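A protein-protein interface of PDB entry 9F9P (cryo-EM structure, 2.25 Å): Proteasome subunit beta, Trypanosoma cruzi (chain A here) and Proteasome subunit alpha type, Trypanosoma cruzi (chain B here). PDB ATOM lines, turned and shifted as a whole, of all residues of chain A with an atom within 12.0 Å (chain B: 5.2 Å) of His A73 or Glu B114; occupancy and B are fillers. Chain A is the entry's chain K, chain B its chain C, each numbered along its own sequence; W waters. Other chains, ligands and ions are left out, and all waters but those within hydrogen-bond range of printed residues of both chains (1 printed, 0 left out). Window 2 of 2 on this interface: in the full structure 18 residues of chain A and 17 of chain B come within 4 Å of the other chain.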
ATOM      1  N   SER A  41      12.346   8.750 -20.990  1.00  0.00           N
ATOM      2  CA  SER A  41      11.986   7.873 -22.099  1.00  0.00           C
ATOM      3  C   SER A  41      12.983   6.707 -22.269  1.00  0.00           C
ATOM      4  O   SER A  41      12.606   5.653 -22.770  1.00  0.00           O
ATOM      5  CB  SER A  41      11.855   8.703 -23.378  1.00  0.00           C
ATOM      6  OG  SER A  41      13.055   9.459 -23.634  1.00  0.00           O
ATOM      7  N   ASN A  64      13.557  16.517  -9.980  1.00  0.00           N
ATOM      8  CA  ASN A  64      14.674  17.341 -10.387  1.00  0.00           C
ATOM      9  C   ASN A  64      15.029  17.117 -11.854  1.00  0.00           C
ATOM     10  O   ASN A  64      15.474  18.027 -12.534  1.00  0.00           O
ATOM     11  CB  ASN A  64      15.851  17.175  -9.428  1.00  0.00           C
ATOM     12  CG  ASN A  64      15.583  17.961  -8.151  1.00  0.00           C
ATOM     13  OD1 ASN A  64      15.862  19.162  -8.074  1.00  0.00           O
ATOM     14  ND2 ASN A  64      14.997  17.316  -7.147  1.00  0.00           N
ATOM     15  N   MET A  65      14.839  15.922 -12.364  1.00  0.00           N
ATOM     16  CA  MET A  65      15.134  15.675 -13.756  1.00  0.00           C
ATOM     17  C   MET A  65      14.114  16.326 -14.684  1.00  0.00           C
ATOM     18  O   MET A  65      14.479  16.690 -15.794  1.00  0.00           O
ATOM     19  CB  MET A  65      15.175  14.174 -14.032  1.00  0.00           C
ATOM     20  CG  MET A  65      16.587  13.617 -13.790  1.00  0.00           C
ATOM     21  SD  MET A  65      16.613  11.822 -13.972  1.00  0.00           S
ATOM     22  CE  MET A  65      16.391  11.694 -15.748  1.00  0.00           C
ATOM     23  N   ALA A  66      12.848  16.417 -14.262  1.00  0.00           N
ATOM     24  CA  ALA A  66      11.811  17.084 -15.041  1.00  0.00           C
ATOM     25  C   ALA A  66      12.024  18.600 -15.054  1.00  0.00           C
ATOM     26  O   ALA A  66      11.989  19.230 -16.094  1.00  0.00           O
ATOM     27  CB  ALA A  66      10.439  16.727 -14.524  1.00  0.00           C
ATOM     28  N   LEU A  67      12.367  19.169 -13.922  1.00  0.00           N
ATOM     29  CA  LEU A  67      12.716  20.576 -13.858  1.00  0.00           C
ATOM     30  C   LEU A  67      13.860  20.877 -14.808  1.00  0.00           C
ATOM     31  O   LEU A  67      13.731  21.712 -15.665  1.00  0.00           O
ATOM     32  CB  LEU A  67      13.127  20.870 -12.412  1.00  0.00           C
ATOM     33  CG  LEU A  67      12.570  22.118 -11.748  1.00  0.00           C
ATOM     34  CD1 LEU A  67      11.155  22.435 -12.210  1.00  0.00           C
ATOM     35  CD2 LEU A  67      12.581  21.903 -10.249  1.00  0.00           C
ATOM     36  N   LYS A  68      14.973  20.164 -14.677  1.00  0.00           N
ATOM     37  CA  LYS A  68      16.125  20.342 -15.545  1.00  0.00           C
ATOM     38  C   LYS A  68      15.773  20.179 -17.010  1.00  0.00           C
ATOM     39  O   LYS A  68      16.427  20.785 -17.826  1.00  0.00           O
ATOM     40  CB  LYS A  68      17.216  19.305 -15.276  1.00  0.00           C
ATOM     41  CG  LYS A  68      18.592  19.740 -15.716  1.00  0.00           C
ATOM     42  CD  LYS A  68      19.589  18.638 -15.921  1.00  0.00           C
ATOM     43  CE  LYS A  68      20.881  19.205 -16.481  1.00  0.00           C
ATOM     44  NZ  LYS A  68      21.879  18.148 -16.772  1.00  0.00           N
ATOM     45  N   ARG A  69      14.778  19.364 -17.336  1.00  0.00           N
ATOM     46  CA  ARG A  69      14.418  19.135 -18.724  1.00  0.00           C
ATOM     47  C   ARG A  69      13.852  20.422 -19.302  1.00  0.00           C
ATOM     48  O   ARG A  69      14.320  20.826 -20.354  1.00  0.00           O
ATOM     49  CB  ARG A  69      13.395  18.001 -18.894  1.00  0.00           C
ATOM     50  CG  ARG A  69      13.768  16.961 -19.940  1.00  0.00           C
ATOM     51  CD  ARG A  69      12.629  16.084 -20.439  1.00  0.00           C
ATOM     52  NE  ARG A  69      11.639  15.656 -19.445  1.00  0.00           N
ATOM     53  CZ  ARG A  69      11.841  14.768 -18.462  1.00  0.00           C
ATOM     54  NH1 ARG A  69      10.829  14.392 -17.700  1.00  0.00           N
ATOM     55  NH2 ARG A  69      13.036  14.242 -18.244  1.00  0.00           N
ATOM     56  N   MET A  70      12.866  21.057 -18.630  1.00  0.00           N
ATOM     57  CA  MET A  70      12.182  22.216 -19.210  1.00  0.00           C
ATOM     58  C   MET A  70      13.014  23.500 -19.170  1.00  0.00           C
ATOM     59  O   MET A  70      12.783  24.390 -19.974  1.00  0.00           O
ATOM     60  CB  MET A  70      10.810  22.534 -18.617  1.00  0.00           C
ATOM     61  CG  MET A  70      10.671  22.250 -17.183  1.00  0.00           C
ATOM     62  SD  MET A  70       8.941  22.331 -16.795  1.00  0.00           S
ATOM     63  CE  MET A  70       8.363  20.800 -17.549  1.00  0.00           C
ATOM     64  N   ARG A  71      14.013  23.594 -18.316  1.00  0.00           N
ATOM     65  CA  ARG A  71      14.970  24.678 -18.438  1.00  0.00           C
ATOM     66  C   ARG A  71      16.112  24.240 -19.352  1.00  0.00           C
ATOM     67  O   ARG A  71      17.283  24.467 -19.036  1.00  0.00           O
ATOM     68  CB  ARG A  71      15.491  25.054 -17.047  1.00  0.00           C
ATOM     69  CG  ARG A  71      14.378  25.246 -16.028  1.00  0.00           C
ATOM     70  CD  ARG A  71      14.833  26.092 -14.858  1.00  0.00           C
ATOM     71  NE  ARG A  71      15.061  25.363 -13.619  1.00  0.00           N
ATOM     72  CZ  ARG A  71      14.316  25.506 -12.527  1.00  0.00           C
ATOM     73  NH1 ARG A  71      14.716  24.970 -11.387  1.00  0.00           N
ATOM     74  NH2 ARG A  71      13.198  26.216 -12.573  1.00  0.00           N
ATOM     75  N   GLU A  72      15.772  23.589 -20.472  1.00  0.00           N
ATOM     76  CA  GLU A  72      16.781  23.078 -21.399  1.00  0.00           C
ATOM     77  C   GLU A  72      16.136  22.594 -22.705  1.00  0.00           C
ATOM     78  O   GLU A  72      16.723  21.777 -23.414  1.00  0.00           O
ATOM     79  CB  GLU A  72      17.594  21.967 -20.730  1.00  0.00           C
ATOM     80  CG  GLU A  72      19.032  21.866 -21.207  1.00  0.00           C
ATOM     81  CD  GLU A  72      20.021  21.293 -20.195  1.00  0.00           C
ATOM     82  OE1 GLU A  72      21.148  20.928 -20.609  1.00  0.00           O
ATOM     83  OE2 GLU A  72      19.688  21.233 -18.995  1.00  0.00           O
ATOM     84  N   HIS A  73      14.941  23.129 -23.016  1.00  0.00           N
ATOM     85  CA  HIS A  73      14.245  22.917 -24.280  1.00  0.00           C
ATOM     86  C   HIS A  73      13.905  21.447 -24.473  1.00  0.00           C
ATOM     87  O   HIS A  73      13.818  20.965 -25.599  1.00  0.00           O
ATOM     88  CB  HIS A  73      15.048  23.446 -25.476  1.00  0.00           C
ATOM     89  CG  HIS A  73      15.554  24.837 -25.296  1.00  0.00           C
ATOM     90  ND1 HIS A  73      14.803  25.844 -24.720  1.00  0.00           N
ATOM     91  CD2 HIS A  73      16.755  25.368 -25.577  1.00  0.00           C
ATOM     92  CE1 HIS A  73      15.533  26.949 -24.673  1.00  0.00           C
ATOM     93  NE2 HIS A  73      16.722  26.681 -25.191  1.00  0.00           N
ATOM     94  N   GLY A  74      13.701  20.745 -23.362  1.00  0.00           N
ATOM     95  CA  GLY A  74      13.105  19.424 -23.407  1.00  0.00           C
ATOM     96  C   GLY A  74      14.052  18.373 -23.962  1.00  0.00           C
ATOM     97  O   GLY A  74      13.598  17.346 -24.454  1.00  0.00           O
ATOM     98  N   ARG A  75      15.355  18.607 -23.809  1.00  0.00           N
ATOM     99  CA  ARG A  75      16.338  17.682 -24.343  1.00  0.00           C
ATOM    100  C   ARG A  75      16.664  16.584 -23.328  1.00  0.00           C
ATOM    101  O   ARG A  75      16.815  16.845 -22.140  1.00  0.00           O
ATOM    102  CB  ARG A  75      17.600  18.432 -24.766  1.00  0.00           C
ATOM    103  CG  ARG A  75      18.033  18.102 -26.190  1.00  0.00           C
ATOM    104  CD  ARG A  75      17.003  18.530 -27.230  1.00  0.00           C
ATOM    105  NE  ARG A  75      17.617  18.951 -28.490  1.00  0.00           N
ATOM    106  CZ  ARG A  75      17.612  20.195 -28.967  1.00  0.00           C
ATOM    107  NH1 ARG A  75      17.019  21.162 -28.289  1.00  0.00           N
ATOM    108  NH2 ARG A  75      18.201  20.471 -30.118  1.00  0.00           N
ATOM    109  N   VAL A  76      16.816  15.357 -23.835  1.00  0.00           N
ATOM    110  CA  VAL A  76      17.126  14.211 -22.997  1.00  0.00           C
ATOM    111  C   VAL A  76      18.528  14.394 -22.417  1.00  0.00           C
ATOM    112  O   VAL A  76      19.502  14.606 -23.136  1.00  0.00           O
ATOM    113  CB  VAL A  76      17.031  12.875 -23.770  1.00  0.00           C
ATOM    114  CG1 VAL A  76      17.132  11.685 -22.825  1.00  0.00           C
ATOM    115  CG2 VAL A  76      15.769  12.757 -24.625  1.00  0.00           C
ATOM    116  N   ILE A  77      18.607  14.245 -21.103  1.00  0.00           N
ATOM    117  CA  ILE A  77      19.842  14.338 -20.354  1.00  0.00           C
ATOM    118  C   ILE A  77      20.635  13.040 -20.472  1.00  0.00           C
ATOM    119  O   ILE A  77      20.070  11.971 -20.577  1.00  0.00           O
ATOM    120  CB  ILE A  77      19.508  14.756 -18.908  1.00  0.00           C
ATOM    121  CG1 ILE A  77      20.245  13.953 -17.844  1.00  0.00           C
ATOM    122  CG2 ILE A  77      18.004  14.737 -18.625  1.00  0.00           C
ATOM    123  CD1 ILE A  77      20.283  14.660 -16.497  1.00  0.00           C
ATOM    124  N   ALA A 113      21.710  10.859 -29.505  1.00  0.00           N
ATOM    125  CA  ALA A 113      22.142  12.179 -29.966  1.00  0.00           C
ATOM    126  C   ALA A 113      21.036  13.236 -29.836  1.00  0.00           C
ATOM    127  O   ALA A 113      19.907  13.028 -30.290  1.00  0.00           O
ATOM    128  CB  ALA A 113      22.625  12.079 -31.396  1.00  0.00           C
ATOM    129  N   ALA A 114      21.397  14.383 -29.229  1.00  0.00           N
ATOM    130  CA  ALA A 114      20.527  15.544 -29.066  1.00  0.00           C
ATOM    131  C   ALA A 114      20.219  16.196 -30.417  1.00  0.00           C
ATOM    132  O   ALA A 114      19.052  16.369 -30.773  1.00  0.00           O
ATOM    133  CB  ALA A 114      21.170  16.557 -28.133  1.00  0.00           C
ATOM    134  N   SER A 115      21.285  16.545 -31.153  1.00  0.00           N
ATOM    135  CA  SER A 115      21.189  17.256 -32.419  1.00  0.00           C
ATOM    136  C   SER A 115      22.273  16.773 -33.389  1.00  0.00           C
ATOM    137  O   SER A 115      22.933  15.761 -33.154  1.00  0.00           O
ATOM    138  CB  SER A 115      21.280  18.749 -32.163  1.00  0.00           C
ATOM    139  OG  SER A 115      22.611  19.167 -31.854  1.00  0.00           O
ATOM    140  N   ASP A 117      24.946  18.613 -34.027  1.00  0.00           N
ATOM    141  CA  ASP A 117      26.203  19.113 -33.469  1.00  0.00           C
ATOM    142  C   ASP A 117      26.758  18.145 -32.418  1.00  0.00           C
ATOM    143  O   ASP A 117      27.935  18.212 -32.059  1.00  0.00           O
ATOM    144  CB  ASP A 117      26.028  20.505 -32.846  1.00  0.00           C
ATOM    145  CG  ASP A 117      25.328  21.518 -33.750  1.00  0.00           C
ATOM    146  OD1 ASP A 117      25.971  21.947 -34.738  1.00  0.00           O
ATOM    147  OD2 ASP A 117      24.130  21.861 -33.471  1.00  0.00           O
ATOM    148  N   ALA B 112      25.058  24.315 -20.296  1.00  0.00           N
ATOM    149  CA  ALA B 112      24.575  24.837 -21.570  1.00  0.00           C
ATOM    150  C   ALA B 112      24.731  26.357 -21.685  1.00  0.00           C
ATOM    151  O   ALA B 112      24.607  27.089 -20.714  1.00  0.00           O
ATOM    152  CB  ALA B 112      23.123  24.456 -21.695  1.00  0.00           C
ATOM    153  N   ALA B 113      24.985  26.859 -22.890  1.00  0.00           N
ATOM    154  CA  ALA B 113      25.227  28.283 -23.057  1.00  0.00           C
ATOM    155  C   ALA B 113      23.970  29.112 -22.731  1.00  0.00           C
ATOM    156  O   ALA B 113      24.047  30.062 -21.964  1.00  0.00           O
ATOM    157  CB  ALA B 113      25.774  28.552 -24.440  1.00  0.00           C
ATOM    158  N   GLU B 114      22.803  28.743 -23.231  1.00  0.00           N
ATOM    159  CA  GLU B 114      21.621  29.531 -22.939  1.00  0.00           C
ATOM    160  C   GLU B 114      21.268  29.532 -21.443  1.00  0.00           C
ATOM    161  O   GLU B 114      20.768  30.512 -20.944  1.00  0.00           O
ATOM    162  CB  GLU B 114      20.415  29.055 -23.747  1.00  0.00           C
ATOM    163  CG  GLU B 114      19.229  30.005 -23.580  1.00  0.00           C
ATOM    164  CD  GLU B 114      18.037  29.855 -24.517  1.00  0.00           C
ATOM    165  OE1 GLU B 114      16.864  29.922 -24.018  1.00  0.00           O
ATOM    166  OE2 GLU B 114      18.269  29.722 -25.750  1.00  0.00           O
ATOM    167  N   ASP B 115      21.561  28.458 -20.725  1.00  0.00           N
ATOM    168  CA  ASP B 115      21.312  28.333 -19.298  1.00  0.00           C
ATOM    169  C   ASP B 115      22.170  29.299 -18.472  1.00  0.00           C
ATOM    170  O   ASP B 115      21.718  29.797 -17.465  1.00  0.00           O
ATOM    171  CB  ASP B 115      21.591  26.888 -18.871  1.00  0.00           C
ATOM    172  CG  ASP B 115      20.824  26.429 -17.637  1.00  0.00           C
ATOM    173  OD1 ASP B 115      19.594  26.719 -17.565  1.00  0.00           O
ATOM    174  OD2 ASP B 115      21.442  25.751 -16.758  1.00  0.00           O
ATOM    175  N   LEU B 116      23.428  29.480 -18.852  1.00  0.00           N
ATOM    176  CA  LEU B 116      24.353  30.353 -18.159  1.00  0.00           C
ATOM    177  C   LEU B 116      23.933  31.797 -18.371  1.00  0.00           C
ATOM    178  O   LEU B 116      23.835  32.585 -17.442  1.00  0.00           O
ATOM    179  CB  LEU B 116      25.764  30.109 -18.678  1.00  0.00           C
ATOM    180  CG  LEU B 116      26.896  30.902 -18.014  1.00  0.00           C
ATOM    181  CD1 LEU B 116      26.970  32.314 -18.550  1.00  0.00           C
ATOM    182  CD2 LEU B 116      26.776  30.899 -16.469  1.00  0.00           C
ATOM    183  N   CYS B 117      23.579  32.103 -19.599  1.00  0.00           N
ATOM    184  CA  CYS B 117      23.016  33.397 -19.944  1.00  0.00           C
ATOM    185  C   CYS B 117      21.742  33.731 -19.159  1.00  0.00           C
ATOM    186  O   CYS B 117      21.535  34.855 -18.731  1.00  0.00           O
ATOM    187  CB  CYS B 117      22.791  33.366 -21.445  1.00  0.00           C
ATOM    188  SG  CYS B 117      22.109  34.903 -22.041  1.00  0.00           S
ATOM    189  N   ARG B 118      20.877  32.752 -18.936  1.00  0.00           N
ATOM    190  CA  ARG B 118      19.631  32.974 -18.203  1.00  0.00           C
ATOM    191  C   ARG B 118      19.895  33.192 -16.703  1.00  0.00           C
ATOM    192  O   ARG B 118      19.243  34.020 -16.107  1.00  0.00           O
ATOM    193  CB  ARG B 118      18.689  31.824 -18.569  1.00  0.00           C
ATOM    194  CG  ARG B 118      17.326  31.821 -17.901  1.00  0.00           C
ATOM    195  CD  ARG B 118      16.523  30.568 -18.240  1.00  0.00           C
ATOM    196  NE  ARG B 118      16.024  29.927 -17.013  1.00  0.00           N
ATOM    197  CZ  ARG B 118      16.756  29.201 -16.149  1.00  0.00           C
ATOM    198  NH1 ARG B 118      16.272  28.897 -14.956  1.00  0.00           N
ATOM    199  NH2 ARG B 118      17.988  28.823 -16.449  1.00  0.00           N
ATOM    200  N   ASP B 146      27.738  24.288 -27.355  1.00  0.00           N
ATOM    201  CA  ASP B 146      27.277  23.109 -26.645  1.00  0.00           C
ATOM    202  C   ASP B 146      26.641  22.099 -27.583  1.00  0.00           C
ATOM    203  O   ASP B 146      26.325  22.425 -28.719  1.00  0.00           O
ATOM    204  CB  ASP B 146      26.330  23.437 -25.491  1.00  0.00           C
ATOM    205  CG  ASP B 146      24.991  24.030 -25.907  1.00  0.00           C
ATOM    206  OD1 ASP B 146      24.456  23.586 -26.917  1.00  0.00           O
ATOM    207  OD2 ASP B 146      24.478  24.920 -25.187  1.00  0.00           O
ATOM    208  N   HIS B 149      22.962  23.051 -29.439  1.00  0.00           N
ATOM    209  CA  HIS B 149      22.734  24.022 -30.498  1.00  0.00           C
ATOM    210  C   HIS B 149      24.021  24.451 -31.189  1.00  0.00           C
ATOM    211  O   HIS B 149      23.975  25.347 -32.010  1.00  0.00           O
ATOM    212  CB  HIS B 149      22.057  25.282 -29.929  1.00  0.00           C
ATOM    213  CG  HIS B 149      20.647  25.050 -29.470  1.00  0.00           C
ATOM    214  ND1 HIS B 149      19.616  24.749 -30.344  1.00  0.00           N
ATOM    215  CD2 HIS B 149      20.100  25.056 -28.225  1.00  0.00           C
ATOM    216  CE1 HIS B 149      18.497  24.539 -29.643  1.00  0.00           C
ATOM    217  NE2 HIS B 149      18.761  24.724 -28.353  1.00  0.00           N
ATOM    218  N   GLN B 152      27.031  29.533 -30.484  1.00  0.00           N
ATOM    219  CA  GLN B 152      26.034  30.535 -30.161  1.00  0.00           C
ATOM    220  C   GLN B 152      26.672  31.863 -29.742  1.00  0.00           C
ATOM    221  O   GLN B 152      27.764  31.907 -29.227  1.00  0.00           O
ATOM    222  CB  GLN B 152      25.176  30.009 -29.021  1.00  0.00           C
ATOM    223  CG  GLN B 152      24.467  28.699 -29.327  1.00  0.00           C
ATOM    224  CD  GLN B 152      24.127  27.921 -28.082  1.00  0.00           C
ATOM    225  OE1 GLN B 152      23.201  28.262 -27.345  1.00  0.00           O
ATOM    226  NE2 GLN B 152      24.868  26.842 -27.858  1.00  0.00           N
ATOM    227  N   TYR B 154      25.217  35.377 -27.733  1.00  0.00           N
ATOM    228  CA  TYR B 154      24.113  36.053 -27.067  1.00  0.00           C
ATOM    229  C   TYR B 154      24.526  37.471 -26.670  1.00  0.00           C
ATOM    230  O   TYR B 154      25.678  37.759 -26.475  1.00  0.00           O
ATOM    231  CB  TYR B 154      23.661  35.302 -25.806  1.00  0.00           C
ATOM    232  CG  TYR B 154      23.017  33.972 -26.064  1.00  0.00           C
ATOM    233  CD1 TYR B 154      21.690  33.859 -26.468  1.00  0.00           C
ATOM    234  CD2 TYR B 154      23.756  32.816 -25.988  1.00  0.00           C
ATOM    235  CE1 TYR B 154      21.105  32.621 -26.719  1.00  0.00           C
ATOM    236  CE2 TYR B 154      23.201  31.577 -26.252  1.00  0.00           C
ATOM    237  CZ  TYR B 154      21.877  31.479 -26.626  1.00  0.00           C
ATOM    238  OH  TYR B 154      21.407  30.219 -26.847  1.00  0.00           O
ATOM    239  N   TYR B 162      17.880  39.130 -22.836  1.00  0.00           N
ATOM    240  CA  TYR B 162      18.932  38.587 -23.659  1.00  0.00           C
ATOM    241  C   TYR B 162      18.362  38.195 -25.006  1.00  0.00           C
ATOM    242  O   TYR B 162      17.196  37.888 -25.094  1.00  0.00           O
ATOM    243  CB  TYR B 162      19.656  37.410 -22.989  1.00  0.00           C
ATOM    244  CG  TYR B 162      18.872  36.139 -22.831  1.00  0.00           C
ATOM    245  CD1 TYR B 162      18.043  35.935 -21.737  1.00  0.00           C
ATOM    246  CD2 TYR B 162      18.979  35.120 -23.759  1.00  0.00           C
ATOM    247  CE1 TYR B 162      17.309  34.766 -21.595  1.00  0.00           C
ATOM    248  CE2 TYR B 162      18.250  33.940 -23.633  1.00  0.00           C
ATOM    249  CZ  TYR B 162      17.399  33.771 -22.558  1.00  0.00           C
ATOM    250  OH  TYR B 162      16.705  32.598 -22.441  1.00  0.00           O
HETATM  251  O   HOH W   1      22.514  23.248 -18.557  1.00  0.00           O
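The side-chain hydroxyl of Ser A115 is in hydrogen-bond range of the backbone NH of Asp A117, at 3.2 Å. The side-chain carboxylate (OE2) of Glu B114 sits at hydrogen-bond distance from the side-chain hydroxyl (OH) of Tyr B154. The side-chain hydroxyl (OH) of Tyr B162 is in hydrogen-bond range of the side-chain carboxylate (OE1) of Glu B114 (3.1 Å). OD1 of Asp B115 lies within salt-bridge range of NH2 of Arg B118 (2.9 Å). OD1 of Asp B146 is in hydrogen-bond range of N of His B149.
Arg A71 touches Asp B115. Arg A71 touches Arg B118 (CD to NH1, 3.2 Å). CD2 of His A73 touches NE2 of His B149, 3.5 Å away. Arg A75 touches His B149 (NH1 to CE1, 3.9 Å). Asp A117 touches His B149 (OD2 to C, 3.5 Å).
Hydrophobic or aromatic side chains of chain A that line the printed part of chain B: His A73. Of the 12 printed residues of chain B, 4 touch a printed residue of chain A. Printed residues of chain B that touch a printed residue of chain A: Glu B114, Asp B115, Arg B118 and His B149. Among the printed residues, no Asp or Glu carboxylate lies within 4 Å of a Lys or Arg side-chain nitrogen of the other chain.
His A73 touches just these residues of chain B: Glu B114 and His B149. Glu B114 touches just one residue of chain A: His A73. No residue of chain A comes within 4 Å of Ala B112. No residue of chain A comes within 4 Å of Cys B117. Arg B118 touches one residue of chain A. Of the printed residues of chain A, His B149 touches His A73 (3.5 Å), Arg A75 (3.9 Å) and Asp A117 (3.5 Å). Printed residues of chain B within 4 Å of Arg A75: His B149 (3.9 Å). Printed residues of chain B within 4 Å of Arg A71: Asp B115 and Arg B118. The nearest printed residue of chain B that does not touch His A73 is Tyr B154 (6.1 Å). The nearest printed residue of chain B that does not touch Arg A75 is Asp B146 (7.7 Å).
Water W1 lies within hydrogen-bond range of the backbone NH of Ala B112 (3.3 Å), the side-chain carboxylate of Asp B115 (3.3 Å) and the side-chain carboxylate of Glu A72 (3.4 Å).
A ring nitrogen (NE2) of His A73 sits close to the side-chain carboxylate of Glu B114 (3.4 Å).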
